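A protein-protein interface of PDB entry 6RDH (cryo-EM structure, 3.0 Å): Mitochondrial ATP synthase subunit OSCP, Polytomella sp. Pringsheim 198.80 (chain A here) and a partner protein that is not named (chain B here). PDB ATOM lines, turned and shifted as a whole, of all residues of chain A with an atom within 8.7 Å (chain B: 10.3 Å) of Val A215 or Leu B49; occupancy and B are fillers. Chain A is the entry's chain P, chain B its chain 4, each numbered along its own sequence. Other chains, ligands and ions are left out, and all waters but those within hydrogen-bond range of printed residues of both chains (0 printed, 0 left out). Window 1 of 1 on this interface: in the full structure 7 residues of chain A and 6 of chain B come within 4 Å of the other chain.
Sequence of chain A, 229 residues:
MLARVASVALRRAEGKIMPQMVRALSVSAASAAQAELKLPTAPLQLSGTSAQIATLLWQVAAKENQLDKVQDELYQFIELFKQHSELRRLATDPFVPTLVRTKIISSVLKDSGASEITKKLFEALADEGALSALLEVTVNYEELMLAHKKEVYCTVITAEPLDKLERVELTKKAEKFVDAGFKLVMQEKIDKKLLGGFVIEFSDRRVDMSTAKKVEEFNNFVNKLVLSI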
ATOM      1  N   LYS A 193      15.270  -5.213 -28.165  1.00  0.00           N
ATOM      2  CA  LYS A 193      15.646  -3.832 -28.417  1.00  0.00           C
ATOM      3  C   LYS A 193      14.515  -3.027 -29.037  1.00  0.00           C
ATOM      4  O   LYS A 193      14.619  -1.800 -29.116  1.00  0.00           O
ATOM      5  CB  LYS A 193      16.903  -3.776 -29.280  1.00  0.00           C
ATOM      6  CG  LYS A 193      18.130  -4.296 -28.548  1.00  0.00           C
ATOM      7  CD  LYS A 193      19.424  -4.037 -29.309  1.00  0.00           C
ATOM      8  CE  LYS A 193      19.603  -4.991 -30.473  1.00  0.00           C
ATOM      9  NZ  LYS A 193      20.928  -4.793 -31.111  1.00  0.00           N
ATOM     10  N   LEU A 195      11.094  -1.762 -27.840  1.00  0.00           N
ATOM     11  CA  LEU A 195      10.440  -1.573 -26.547  1.00  0.00           C
ATOM     12  C   LEU A 195       8.924  -1.608 -26.706  1.00  0.00           C
ATOM     13  O   LEU A 195       8.222  -0.652 -26.405  1.00  0.00           O
ATOM     14  CB  LEU A 195      10.891  -0.262 -25.909  1.00  0.00           C
ATOM     15  CG  LEU A 195      12.181  -0.214 -25.091  1.00  0.00           C
ATOM     16  CD1 LEU A 195      12.104  -1.237 -23.974  1.00  0.00           C
ATOM     17  CD2 LEU A 195      13.440  -0.390 -25.921  1.00  0.00           C
ATOM     18  N   ASP A 208       7.369  -0.096 -39.307  1.00  0.00           N
ATOM     19  CA  ASP A 208       7.941  -0.040 -37.967  1.00  0.00           C
ATOM     20  C   ASP A 208       6.936   0.649 -37.049  1.00  0.00           C
ATOM     21  O   ASP A 208       6.963   1.867 -36.880  1.00  0.00           O
ATOM     22  CB  ASP A 208       9.267   0.695 -37.984  1.00  0.00           C
ATOM     23  CG  ASP A 208      10.188   0.261 -36.873  1.00  0.00           C
ATOM     24  OD1 ASP A 208       9.737   0.206 -35.715  1.00  0.00           O
ATOM     25  OD2 ASP A 208      11.367  -0.023 -37.156  1.00  0.00           O
ATOM     26  N   MET A 209       6.049  -0.141 -36.452  1.00  0.00           N
ATOM     27  CA  MET A 209       5.105   0.374 -35.476  1.00  0.00           C
ATOM     28  C   MET A 209       5.603   0.184 -34.052  1.00  0.00           C
ATOM     29  O   MET A 209       4.826   0.322 -33.104  1.00  0.00           O
ATOM     30  CB  MET A 209       3.739  -0.279 -35.667  1.00  0.00           C
ATOM     31  CG  MET A 209       3.133   0.023 -37.017  1.00  0.00           C
ATOM     32  SD  MET A 209       1.471  -0.605 -37.295  1.00  0.00           S
ATOM     33  CE  MET A 209       0.522   0.495 -36.249  1.00  0.00           C
ATOM     34  N   SER A 210       6.887  -0.122 -33.890  1.00  0.00           N
ATOM     35  CA  SER A 210       7.485  -0.285 -32.577  1.00  0.00           C
ATOM     36  C   SER A 210       7.597   1.058 -31.874  1.00  0.00           C
ATOM     37  O   SER A 210       7.564   2.119 -32.497  1.00  0.00           O
ATOM     38  CB  SER A 210       8.867  -0.914 -32.695  1.00  0.00           C
ATOM     39  OG  SER A 210       9.843   0.077 -32.947  1.00  0.00           O
ATOM     40  N   THR A 211       7.734   1.006 -30.553  1.00  0.00           N
ATOM     41  CA  THR A 211       7.802   2.235 -29.781  1.00  0.00           C
ATOM     42  C   THR A 211       9.217   2.744 -29.601  1.00  0.00           C
ATOM     43  O   THR A 211       9.385   3.889 -29.188  1.00  0.00           O
ATOM     44  CB  THR A 211       7.171   2.060 -28.400  1.00  0.00           C
ATOM     45  OG1 THR A 211       8.029   1.258 -27.587  1.00  0.00           O
ATOM     46  CG2 THR A 211       5.817   1.391 -28.519  1.00  0.00           C
ATOM     47  N   ALA A 212      10.237   1.937 -29.887  1.00  0.00           N
ATOM     48  CA  ALA A 212      11.586   2.486 -29.953  1.00  0.00           C
ATOM     49  C   ALA A 212      11.711   3.452 -31.122  1.00  0.00           C
ATOM     50  O   ALA A 212      12.293   4.537 -30.988  1.00  0.00           O
ATOM     51  CB  ALA A 212      12.607   1.361 -30.069  1.00  0.00           C
ATOM     52  N   LYS A 213      11.121   3.085 -32.261  1.00  0.00           N
ATOM     53  CA  LYS A 213      11.016   3.994 -33.393  1.00  0.00           C
ATOM     54  C   LYS A 213      10.180   5.214 -33.047  1.00  0.00           C
ATOM     55  O   LYS A 213      10.509   6.329 -33.461  1.00  0.00           O
ATOM     56  CB  LYS A 213      10.406   3.271 -34.588  1.00  0.00           C
ATOM     57  CG  LYS A 213      10.649   3.942 -35.920  1.00  0.00           C
ATOM     58  CD  LYS A 213      12.034   3.622 -36.421  1.00  0.00           C
ATOM     59  CE  LYS A 213      12.300   4.268 -37.754  1.00  0.00           C
ATOM     60  NZ  LYS A 213      13.658   3.909 -38.230  1.00  0.00           N
ATOM     61  N   LYS A 214       9.112   5.021 -32.272  1.00  0.00           N
ATOM     62  CA  LYS A 214       8.242   6.133 -31.914  1.00  0.00           C
ATOM     63  C   LYS A 214       8.943   7.113 -30.986  1.00  0.00           C
ATOM     64  O   LYS A 214       8.817   8.328 -31.162  1.00  0.00           O
ATOM     65  CB  LYS A 214       6.959   5.614 -31.273  1.00  0.00           C
ATOM     66  CG  LYS A 214       5.947   6.698 -30.953  1.00  0.00           C
ATOM     67  CD  LYS A 214       4.721   6.110 -30.290  1.00  0.00           C
ATOM     68  CE  LYS A 214       3.694   7.176 -29.952  1.00  0.00           C
ATOM     69  NZ  LYS A 214       3.190   7.890 -31.153  1.00  0.00           N
ATOM     70  N   VAL A 215       9.724   6.619 -30.025  1.00  0.00           N
ATOM     71  CA  VAL A 215      10.405   7.558 -29.145  1.00  0.00           C
ATOM     72  C   VAL A 215      11.588   8.208 -29.839  1.00  0.00           C
ATOM     73  O   VAL A 215      11.882   9.377 -29.571  1.00  0.00           O
ATOM     74  CB  VAL A 215      10.814   6.917 -27.805  1.00  0.00           C
ATOM     75  CG1 VAL A 215       9.607   6.348 -27.106  1.00  0.00           C
ATOM     76  CG2 VAL A 215      11.857   5.844 -27.984  1.00  0.00           C
ATOM     77  N   GLU A 216      12.248   7.530 -30.789  1.00  0.00           N
ATOM     78  CA  GLU A 216      13.330   8.230 -31.474  1.00  0.00           C
ATOM     79  C   GLU A 216      12.798   9.235 -32.490  1.00  0.00           C
ATOM     80  O   GLU A 216      13.399  10.302 -32.665  1.00  0.00           O
ATOM     81  CB  GLU A 216      14.306   7.236 -32.111  1.00  0.00           C
ATOM     82  CG  GLU A 216      13.963   6.713 -33.484  1.00  0.00           C
ATOM     83  CD  GLU A 216      15.090   5.900 -34.079  1.00  0.00           C
ATOM     84  OE1 GLU A 216      16.243   6.378 -34.042  1.00  0.00           O
ATOM     85  OE2 GLU A 216      14.828   4.789 -34.584  1.00  0.00           O
ATOM     86  N   GLU A 217      11.635   8.975 -33.092  1.00  0.00           N
ATOM     87  CA  GLU A 217      11.047   9.953 -33.994  1.00  0.00           C
ATOM     88  C   GLU A 217      10.461  11.121 -33.217  1.00  0.00           C
ATOM     89  O   GLU A 217      10.527  12.270 -33.667  1.00  0.00           O
ATOM     90  CB  GLU A 217       9.985   9.284 -34.862  1.00  0.00           C
ATOM     91  CG  GLU A 217       9.411  10.180 -35.943  1.00  0.00           C
ATOM     92  CD  GLU A 217      10.431  10.550 -37.012  1.00  0.00           C
ATOM     93  OE1 GLU A 217      11.357   9.751 -37.271  1.00  0.00           O
ATOM     94  OE2 GLU A 217      10.317  11.655 -37.584  1.00  0.00           O
ATOM     95  N   PHE A 218       9.915  10.845 -32.028  1.00  0.00           N
ATOM     96  CA  PHE A 218       9.450  11.888 -31.124  1.00  0.00           C
ATOM     97  C   PHE A 218      10.597  12.785 -30.687  1.00  0.00           C
ATOM     98  O   PHE A 218      10.457  14.013 -30.643  1.00  0.00           O
ATOM     99  CB  PHE A 218       8.780  11.228 -29.919  1.00  0.00           C
ATOM    100  CG  PHE A 218       8.443  12.168 -28.800  1.00  0.00           C
ATOM    101  CD1 PHE A 218       9.271  12.281 -27.694  1.00  0.00           C
ATOM    102  CD2 PHE A 218       7.274  12.895 -28.823  1.00  0.00           C
ATOM    103  CE1 PHE A 218       8.963  13.132 -26.674  1.00  0.00           C
ATOM    104  CE2 PHE A 218       6.960  13.734 -27.792  1.00  0.00           C
ATOM    105  CZ  PHE A 218       7.804  13.857 -26.724  1.00  0.00           C
ATOM    106  N   ASN A 219      11.739  12.181 -30.347  1.00  0.00           N
ATOM    107  CA  ASN A 219      12.899  12.962 -29.949  1.00  0.00           C
ATOM    108  C   ASN A 219      13.434  13.786 -31.108  1.00  0.00           C
ATOM    109  O   ASN A 219      13.827  14.936 -30.907  1.00  0.00           O
ATOM    110  CB  ASN A 219      13.986  12.053 -29.395  1.00  0.00           C
ATOM    111  CG  ASN A 219      13.627  11.481 -28.052  1.00  0.00           C
ATOM    112  OD1 ASN A 219      12.640  11.880 -27.444  1.00  0.00           O
ATOM    113  ND2 ASN A 219      14.432  10.546 -27.573  1.00  0.00           N
ATOM    114  N   ASN A 220      13.431  13.233 -32.327  1.00  0.00           N
ATOM    115  CA  ASN A 220      13.843  14.016 -33.493  1.00  0.00           C
ATOM    116  C   ASN A 220      12.903  15.189 -33.733  1.00  0.00           C
ATOM    117  O   ASN A 220      13.356  16.301 -34.026  1.00  0.00           O
ATOM    118  CB  ASN A 220      13.910  13.138 -34.739  1.00  0.00           C
ATOM    119  CG  ASN A 220      15.125  12.245 -34.755  1.00  0.00           C
ATOM    120  OD1 ASN A 220      15.131  11.197 -35.397  1.00  0.00           O
ATOM    121  ND2 ASN A 220      16.161  12.648 -34.036  1.00  0.00           N
ATOM    122  N   PHE A 221      11.602  14.971 -33.542  1.00  0.00           N
ATOM    123  CA  PHE A 221      10.622  16.032 -33.728  1.00  0.00           C
ATOM    124  C   PHE A 221      10.795  17.152 -32.711  1.00  0.00           C
ATOM    125  O   PHE A 221      10.786  18.334 -33.075  1.00  0.00           O
ATOM    126  CB  PHE A 221       9.216  15.453 -33.635  1.00  0.00           C
ATOM    127  CG  PHE A 221       8.141  16.444 -33.916  1.00  0.00           C
ATOM    128  CD1 PHE A 221       7.871  16.831 -35.212  1.00  0.00           C
ATOM    129  CD2 PHE A 221       7.397  16.989 -32.891  1.00  0.00           C
ATOM    130  CE1 PHE A 221       6.879  17.742 -35.478  1.00  0.00           C
ATOM    131  CE2 PHE A 221       6.406  17.901 -33.154  1.00  0.00           C
ATOM    132  CZ  PHE A 221       6.147  18.276 -34.446  1.00  0.00           C
ATOM    133  N   VAL A 222      10.951  16.813 -31.433  1.00  0.00           N
ATOM    134  CA  VAL A 222      10.994  17.863 -30.422  1.00  0.00           C
ATOM    135  C   VAL A 222      12.374  18.506 -30.366  1.00  0.00           C
ATOM    136  O   VAL A 222      12.511  19.662 -29.955  1.00  0.00           O
ATOM    137  CB  VAL A 222      10.545  17.334 -29.049  1.00  0.00           C
ATOM    138  CG1 VAL A 222       9.145  16.787 -29.149  1.00  0.00           C
ATOM    139  CG2 VAL A 222      11.499  16.301 -28.510  1.00  0.00           C
ATOM    140  N   ASN A 223      13.418  17.787 -30.790  1.00  0.00           N
ATOM    141  CA  ASN A 223      14.725  18.417 -30.892  1.00  0.00           C
ATOM    142  C   ASN A 223      14.862  19.239 -32.157  1.00  0.00           C
ATOM    143  O   ASN A 223      15.783  20.052 -32.250  1.00  0.00           O
ATOM    144  CB  ASN A 223      15.835  17.375 -30.828  1.00  0.00           C
ATOM    145  CG  ASN A 223      15.897  16.679 -29.495  1.00  0.00           C
ATOM    146  OD1 ASN A 223      15.296  17.125 -28.522  1.00  0.00           O
ATOM    147  ND2 ASN A 223      16.621  15.570 -29.442  1.00  0.00           N
ATOM    148  N   LYS B   9      -1.578  23.552 -15.026  1.00  0.00           N
ATOM    149  CA  LYS B   9      -0.498  22.621 -14.768  1.00  0.00           C
ATOM    150  C   LYS B   9       0.772  23.343 -14.382  1.00  0.00           C
ATOM    151  O   LYS B   9       1.638  22.744 -13.743  1.00  0.00           O
ATOM    152  CB  LYS B   9      -0.233  21.735 -15.987  1.00  0.00           C
ATOM    153  CG  LYS B   9       0.075  20.304 -15.625  1.00  0.00           C
ATOM    154  CD  LYS B   9      -0.280  19.371 -16.760  1.00  0.00           C
ATOM    155  CE  LYS B   9      -0.120  17.924 -16.343  1.00  0.00           C
ATOM    156  NZ  LYS B   9      -0.652  16.976 -17.361  1.00  0.00           N
ATOM    157  N   ASP B  45      -4.681  12.734 -19.574  1.00  0.00           N
ATOM    158  CA  ASP B  45      -4.361  12.456 -20.968  1.00  0.00           C
ATOM    159  C   ASP B  45      -2.881  12.799 -21.130  1.00  0.00           C
ATOM    160  O   ASP B  45      -2.155  12.859 -20.131  1.00  0.00           O
ATOM    161  CB  ASP B  45      -5.327  13.239 -21.880  1.00  0.00           C
ATOM    162  CG  ASP B  45      -5.360  12.719 -23.306  1.00  0.00           C
ATOM    163  OD1 ASP B  45      -6.019  13.352 -24.157  1.00  0.00           O
ATOM    164  OD2 ASP B  45      -4.717  11.683 -23.571  1.00  0.00           O
ATOM    165  N   ALA B  46      -2.433  12.994 -22.379  1.00  0.00           N
ATOM    166  CA  ALA B  46      -1.055  13.352 -22.732  1.00  0.00           C
ATOM    167  C   ALA B  46      -0.075  12.279 -22.249  1.00  0.00           C
ATOM    168  O   ALA B  46       0.628  12.430 -21.251  1.00  0.00           O
ATOM    169  CB  ALA B  46      -0.673  14.749 -22.217  1.00  0.00           C
ATOM    170  N   SER B  47      -0.117  11.155 -22.966  1.00  0.00           N
ATOM    171  CA  SER B  47       0.616   9.929 -22.667  1.00  0.00           C
ATOM    172  C   SER B  47       2.124  10.114 -22.548  1.00  0.00           C
ATOM    173  O   SER B  47       2.649  11.146 -22.974  1.00  0.00           O
ATOM    174  CB  SER B  47       0.325   8.895 -23.751  1.00  0.00           C
ATOM    175  OG  SER B  47       0.472   9.484 -25.030  1.00  0.00           O
ATOM    176  N   GLU B  48       2.801   9.049 -22.080  1.00  0.00           N
ATOM    177  CA  GLU B  48       4.089   9.096 -21.370  1.00  0.00           C
ATOM    178  C   GLU B  48       5.135  10.010 -21.998  1.00  0.00           C
ATOM    179  O   GLU B  48       5.919  10.643 -21.283  1.00  0.00           O
ATOM    180  CB  GLU B  48       4.662   7.686 -21.262  1.00  0.00           C
ATOM    181  CG  GLU B  48       4.245   6.934 -20.019  1.00  0.00           C
ATOM    182  CD  GLU B  48       4.331   5.437 -20.202  1.00  0.00           C
ATOM    183  OE1 GLU B  48       4.585   4.726 -19.208  1.00  0.00           O
ATOM    184  OE2 GLU B  48       4.147   4.971 -21.345  1.00  0.00           O
ATOM    185  N   LEU B  49       5.163  10.095 -23.326  1.00  0.00           N
ATOM    186  CA  LEU B  49       6.119  10.982 -23.973  1.00  0.00           C
ATOM    187  C   LEU B  49       5.738  12.442 -23.778  1.00  0.00           C
ATOM    188  O   LEU B  49       6.591  13.262 -23.424  1.00  0.00           O
ATOM    189  CB  LEU B  49       6.226  10.640 -25.453  1.00  0.00           C
ATOM    190  CG  LEU B  49       6.788   9.251 -25.742  1.00  0.00           C
ATOM    191  CD1 LEU B  49       6.927   9.047 -27.229  1.00  0.00           C
ATOM    192  CD2 LEU B  49       8.118   9.069 -25.047  1.00  0.00           C
ATOM    193  N   ILE B  50       4.461  12.780 -23.979  1.00  0.00           N
ATOM    194  CA  ILE B  50       4.010  14.149 -23.744  1.00  0.00           C
ATOM    195  C   ILE B  50       4.053  14.476 -22.263  1.00  0.00           C
ATOM    196  O   ILE B  50       4.326  15.618 -21.884  1.00  0.00           O
ATOM    197  CB  ILE B  50       2.598  14.373 -24.313  1.00  0.00           C
ATOM    198  CG1 ILE B  50       2.449  13.706 -25.672  1.00  0.00           C
ATOM    199  CG2 ILE B  50       2.293  15.854 -24.432  1.00  0.00           C
ATOM    200  CD1 ILE B  50       3.258  14.346 -26.760  1.00  0.00           C
ATOM    201  N   ALA B  51       3.832  13.481 -21.404  1.00  0.00           N
ATOM    202  CA  ALA B  51       3.899  13.714 -19.968  1.00  0.00           C
ATOM    203  C   ALA B  51       5.323  13.999 -19.522  1.00  0.00           C
ATOM    204  O   ALA B  51       5.559  14.921 -18.740  1.00  0.00           O
ATOM    205  CB  ALA B  51       3.334  12.517 -19.212  1.00  0.00           C
ATOM    206  N   GLN B  52       6.294  13.246 -20.036  1.00  0.00           N
ATOM    207  CA  GLN B  52       7.677  13.506 -19.670  1.00  0.00           C
ATOM    208  C   GLN B  52       8.213  14.783 -20.296  1.00  0.00           C
ATOM    209  O   GLN B  52       9.012  15.477 -19.659  1.00  0.00           O
ATOM    210  CB  GLN B  52       8.567  12.329 -20.066  1.00  0.00           C
ATOM    211  CG  GLN B  52       8.550  11.163 -19.083  1.00  0.00           C
ATOM    212  CD  GLN B  52       9.170  11.484 -17.727  1.00  0.00           C
ATOM    213  OE1 GLN B  52       9.928  12.443 -17.578  1.00  0.00           O
ATOM    214  NE2 GLN B  52       8.844  10.673 -16.729  1.00  0.00           N
ATOM    215  N   LEU B  53       7.751  15.138 -21.495  1.00  0.00           N
ATOM    216  CA  LEU B  53       8.164  16.398 -22.101  1.00  0.00           C
ATOM    217  C   LEU B  53       7.570  17.589 -21.361  1.00  0.00           C
ATOM    218  O   LEU B  53       8.248  18.601 -21.152  1.00  0.00           O
ATOM    219  CB  LEU B  53       7.751  16.423 -23.565  1.00  0.00           C
ATOM    220  CG  LEU B  53       8.280  17.590 -24.377  1.00  0.00           C
ATOM    221  CD1 LEU B  53       9.763  17.448 -24.528  1.00  0.00           C
ATOM    222  CD2 LEU B  53       7.611  17.616 -25.720  1.00  0.00           C
ATOM    223  N   GLU B  54       6.315  17.477 -20.933  1.00  0.00           N
ATOM    224  CA  GLU B  54       5.696  18.552 -20.178  1.00  0.00           C
ATOM    225  C   GLU B  54       6.275  18.652 -18.775  1.00  0.00           C
ATOM    226  O   GLU B  54       6.369  19.752 -18.235  1.00  0.00           O
ATOM    227  CB  GLU B  54       4.189  18.340 -20.135  1.00  0.00           C
ATOM    228  CG  GLU B  54       3.397  19.554 -19.738  1.00  0.00           C
ATOM    229  CD  GLU B  54       1.916  19.354 -19.947  1.00  0.00           C
ATOM    230  OE1 GLU B  54       1.533  18.268 -20.425  1.00  0.00           O
ATOM    231  OE2 GLU B  54       1.134  20.274 -19.631  1.00  0.00           O
ATOM    232  N   LYS B  55       6.694  17.532 -18.184  1.00  0.00           N
ATOM    233  CA  LYS B  55       7.433  17.592 -16.927  1.00  0.00           C
ATOM    234  C   LYS B  55       8.768  18.288 -17.107  1.00  0.00           C
ATOM    235  O   LYS B  55       9.178  19.081 -16.254  1.00  0.00           O
ATOM    236  CB  LYS B  55       7.668  16.190 -16.378  1.00  0.00           C
ATOM    237  CG  LYS B  55       6.674  15.748 -15.346  1.00  0.00           C
ATOM    238  CD  LYS B  55       7.240  14.627 -14.502  1.00  0.00           C
ATOM    239  CE  LYS B  55       8.470  15.060 -13.738  1.00  0.00           C
ATOM    240  NZ  LYS B  55       8.991  13.933 -12.923  1.00  0.00           N
ATOM    241  N   LYS B  56       9.456  18.000 -18.213  1.00  0.00           N
ATOM    242  CA  LYS B  56      10.749  18.615 -18.487  1.00  0.00           C
ATOM    243  C   LYS B  56      10.615  20.115 -18.682  1.00  0.00           C
ATOM    244  O   LYS B  56      11.462  20.885 -18.224  1.00  0.00           O
ATOM    245  CB  LYS B  56      11.365  17.962 -19.721  1.00  0.00           C
ATOM    246  CG  LYS B  56      12.705  18.500 -20.145  1.00  0.00           C
ATOM    247  CD  LYS B  56      13.170  17.794 -21.393  1.00  0.00           C
ATOM    248  CE  LYS B  56      14.523  18.291 -21.825  1.00  0.00           C
ATOM    249  NZ  LYS B  56      15.080  17.474 -22.932  1.00  0.00           N
ATOM    250  N   TYR B  57       9.547  20.549 -19.326  1.00  0.00           N
ATOM    251  CA  TYR B  57       9.377  21.968 -19.586  1.00  0.00           C
ATOM    252  C   TYR B  57       8.584  22.695 -18.512  1.00  0.00           C
ATOM    253  O   TYR B  57       8.450  23.916 -18.583  1.00  0.00           O
ATOM    254  CB  TYR B  57       8.724  22.164 -20.944  1.00  0.00           C
ATOM    255  CG  TYR B  57       9.748  22.200 -22.026  1.00  0.00           C
ATOM    256  CD1 TYR B  57      10.056  21.067 -22.747  1.00  0.00           C
ATOM    257  CD2 TYR B  57      10.443  23.358 -22.296  1.00  0.00           C
ATOM    258  CE1 TYR B  57      11.010  21.092 -23.722  1.00  0.00           C
ATOM    259  CE2 TYR B  57      11.400  23.392 -23.262  1.00  0.00           C
ATOM    260  CZ  TYR B  57      11.675  22.259 -23.980  1.00  0.00           C
ATOM    261  OH  TYR B  57      12.635  22.293 -24.957  1.00  0.00           O
ATOM    262  N   GLN B 111      17.032   4.124 -17.537  1.00  0.00           N
ATOM    263  CA  GLN B 111      16.241   4.433 -18.717  1.00  0.00           C
ATOM    264  C   GLN B 111      17.066   4.300 -19.987  1.00  0.00           C
ATOM    265  O   GLN B 111      16.548   3.867 -21.020  1.00  0.00           O
ATOM    266  CB  GLN B 111      15.666   5.842 -18.585  1.00  0.00           C
ATOM    267  CG  GLN B 111      14.831   6.315 -19.749  1.00  0.00           C
ATOM    268  CD  GLN B 111      14.256   7.688 -19.510  1.00  0.00           C
ATOM    269  OE1 GLN B 111      14.016   8.079 -18.369  1.00  0.00           O
ATOM    270  NE2 GLN B 111      14.033   8.432 -20.584  1.00  0.00           N
ATOM    271  N   GLU B 112      18.353   4.653 -19.927  1.00  0.00           N
ATOM    272  CA  GLU B 112      19.198   4.571 -21.116  1.00  0.00           C
ATOM    273  C   GLU B 112      19.484   3.125 -21.500  1.00  0.00           C
ATOM    274  O   GLU B 112      19.405   2.758 -22.677  1.00  0.00           O
ATOM    275  CB  GLU B 112      20.506   5.325 -20.889  1.00  0.00           C
ATOM    276  CG  GLU B 112      20.386   6.819 -21.061  1.00  0.00           C
ATOM    277  CD  GLU B 112      20.072   7.216 -22.478  1.00  0.00           C
ATOM    278  OE1 GLU B 112      20.621   6.594 -23.406  1.00  0.00           O
ATOM    279  OE2 GLU B 112      19.264   8.146 -22.666  1.00  0.00           O
ATOM    280  N   THR B 115      17.611  -1.471 -22.626  1.00  0.00           N
ATOM    281  CA  THR B 115      17.558  -2.202 -23.883  1.00  0.00           C
ATOM    282  C   THR B 115      18.886  -2.816 -24.301  1.00  0.00           C
ATOM    283  O   THR B 115      19.004  -3.278 -25.441  1.00  0.00           O
ATOM    284  CB  THR B 115      17.071  -1.269 -24.989  1.00  0.00           C
ATOM    285  OG1 THR B 115      17.120  -1.960 -26.235  1.00  0.00           O
ATOM    286  CG2 THR B 115      17.947  -0.027 -25.063  1.00  0.00           C
ATOM    287  N   LYS B 125      26.239   3.725 -24.219  1.00  0.00           N
ATOM    288  CA  LYS B 125      24.979   4.441 -24.068  1.00  0.00           C
ATOM    289  C   LYS B 125      24.954   5.394 -22.884  1.00  0.00           C
ATOM    290  O   LYS B 125      24.296   6.434 -22.961  1.00  0.00           O
ATOM    291  CB  LYS B 125      23.819   3.455 -23.953  1.00  0.00           C
ATOM    292  CG  LYS B 125      23.439   2.832 -25.274  1.00  0.00           C
ATOM    293  CD  LYS B 125      21.958   2.553 -25.315  1.00  0.00           C
ATOM    294  CE  LYS B 125      21.169   3.847 -25.269  1.00  0.00           C
ATOM    295  NZ  LYS B 125      19.724   3.603 -25.013  1.00  0.00           N
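Among the printed residues, pairs that only touch across the chains: Lys A193 with Thr B115 (3.2 Å), Leu A195 with Thr B115 (3.9 Å), Val A215 with Leu B49 (3.7 Å), Phe A218 with Leu B49 (3.6 Å), Phe A218 with Ile B50 (3.9 Å), Phe A218 with Leu B53 (3.9 Å) and Val A222 with Leu B53 (3.8 Å).
The backbone carbonyl oxygen (O) of Val A215 sits close to the side-chain amide oxygen (OD1) of Asn A219.
Hydrophobic or aromatic side chains of chain B that line the printed part of chain A: Leu B49, Ile B50 and Leu B53.
Of the 18 printed residues of chain A, 5 touch a printed residue of chain B.
Printed residues of chain A that touch a printed residue of chain B: Lys A193, Leu A195, Val A215, Phe A218 and Val A222.
Hydrophobic or aromatic side chains of chain A within 4 Å of the printed part of chain B: Leu A195, Val A215, Phe A218 and Val A222.
Among the printed residues, 7 pairs touch across the chains.
Among the printed residues, no Asp or Glu carboxylate lies within 4 Å of a Lys or Arg side-chain nitrogen of the other chain.
Of the printed residues of chain B, Val A215 touches Leu B49 (3.7 Å).
Leu B49 touches just these residues of chain A: Val A215 (3.7 Å) and Phe A218 (3.6 Å).
No residue of chain B comes within 4 Å of Ala A212.
No residue of chain B comes within 4 Å of Lys A214.
Phe A218 touches three residues of chain B.
Of the printed residues of chain B, Val A222 touches Leu B53 (3.8 Å).
Printed residues of chain A within 4 Å of Ile B50: Phe A218 (3.9 Å).
Lys B9 touches none of the printed residues of chain A.
Phe A221 touches none of the printed residues of chain B.
The nearest residue of chain B that does not touch Val A215 is Glu B48 (7.7 Å).
The nearest residue of chain A that does not touch Leu B49 is Lys A214 (4.4 Å).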
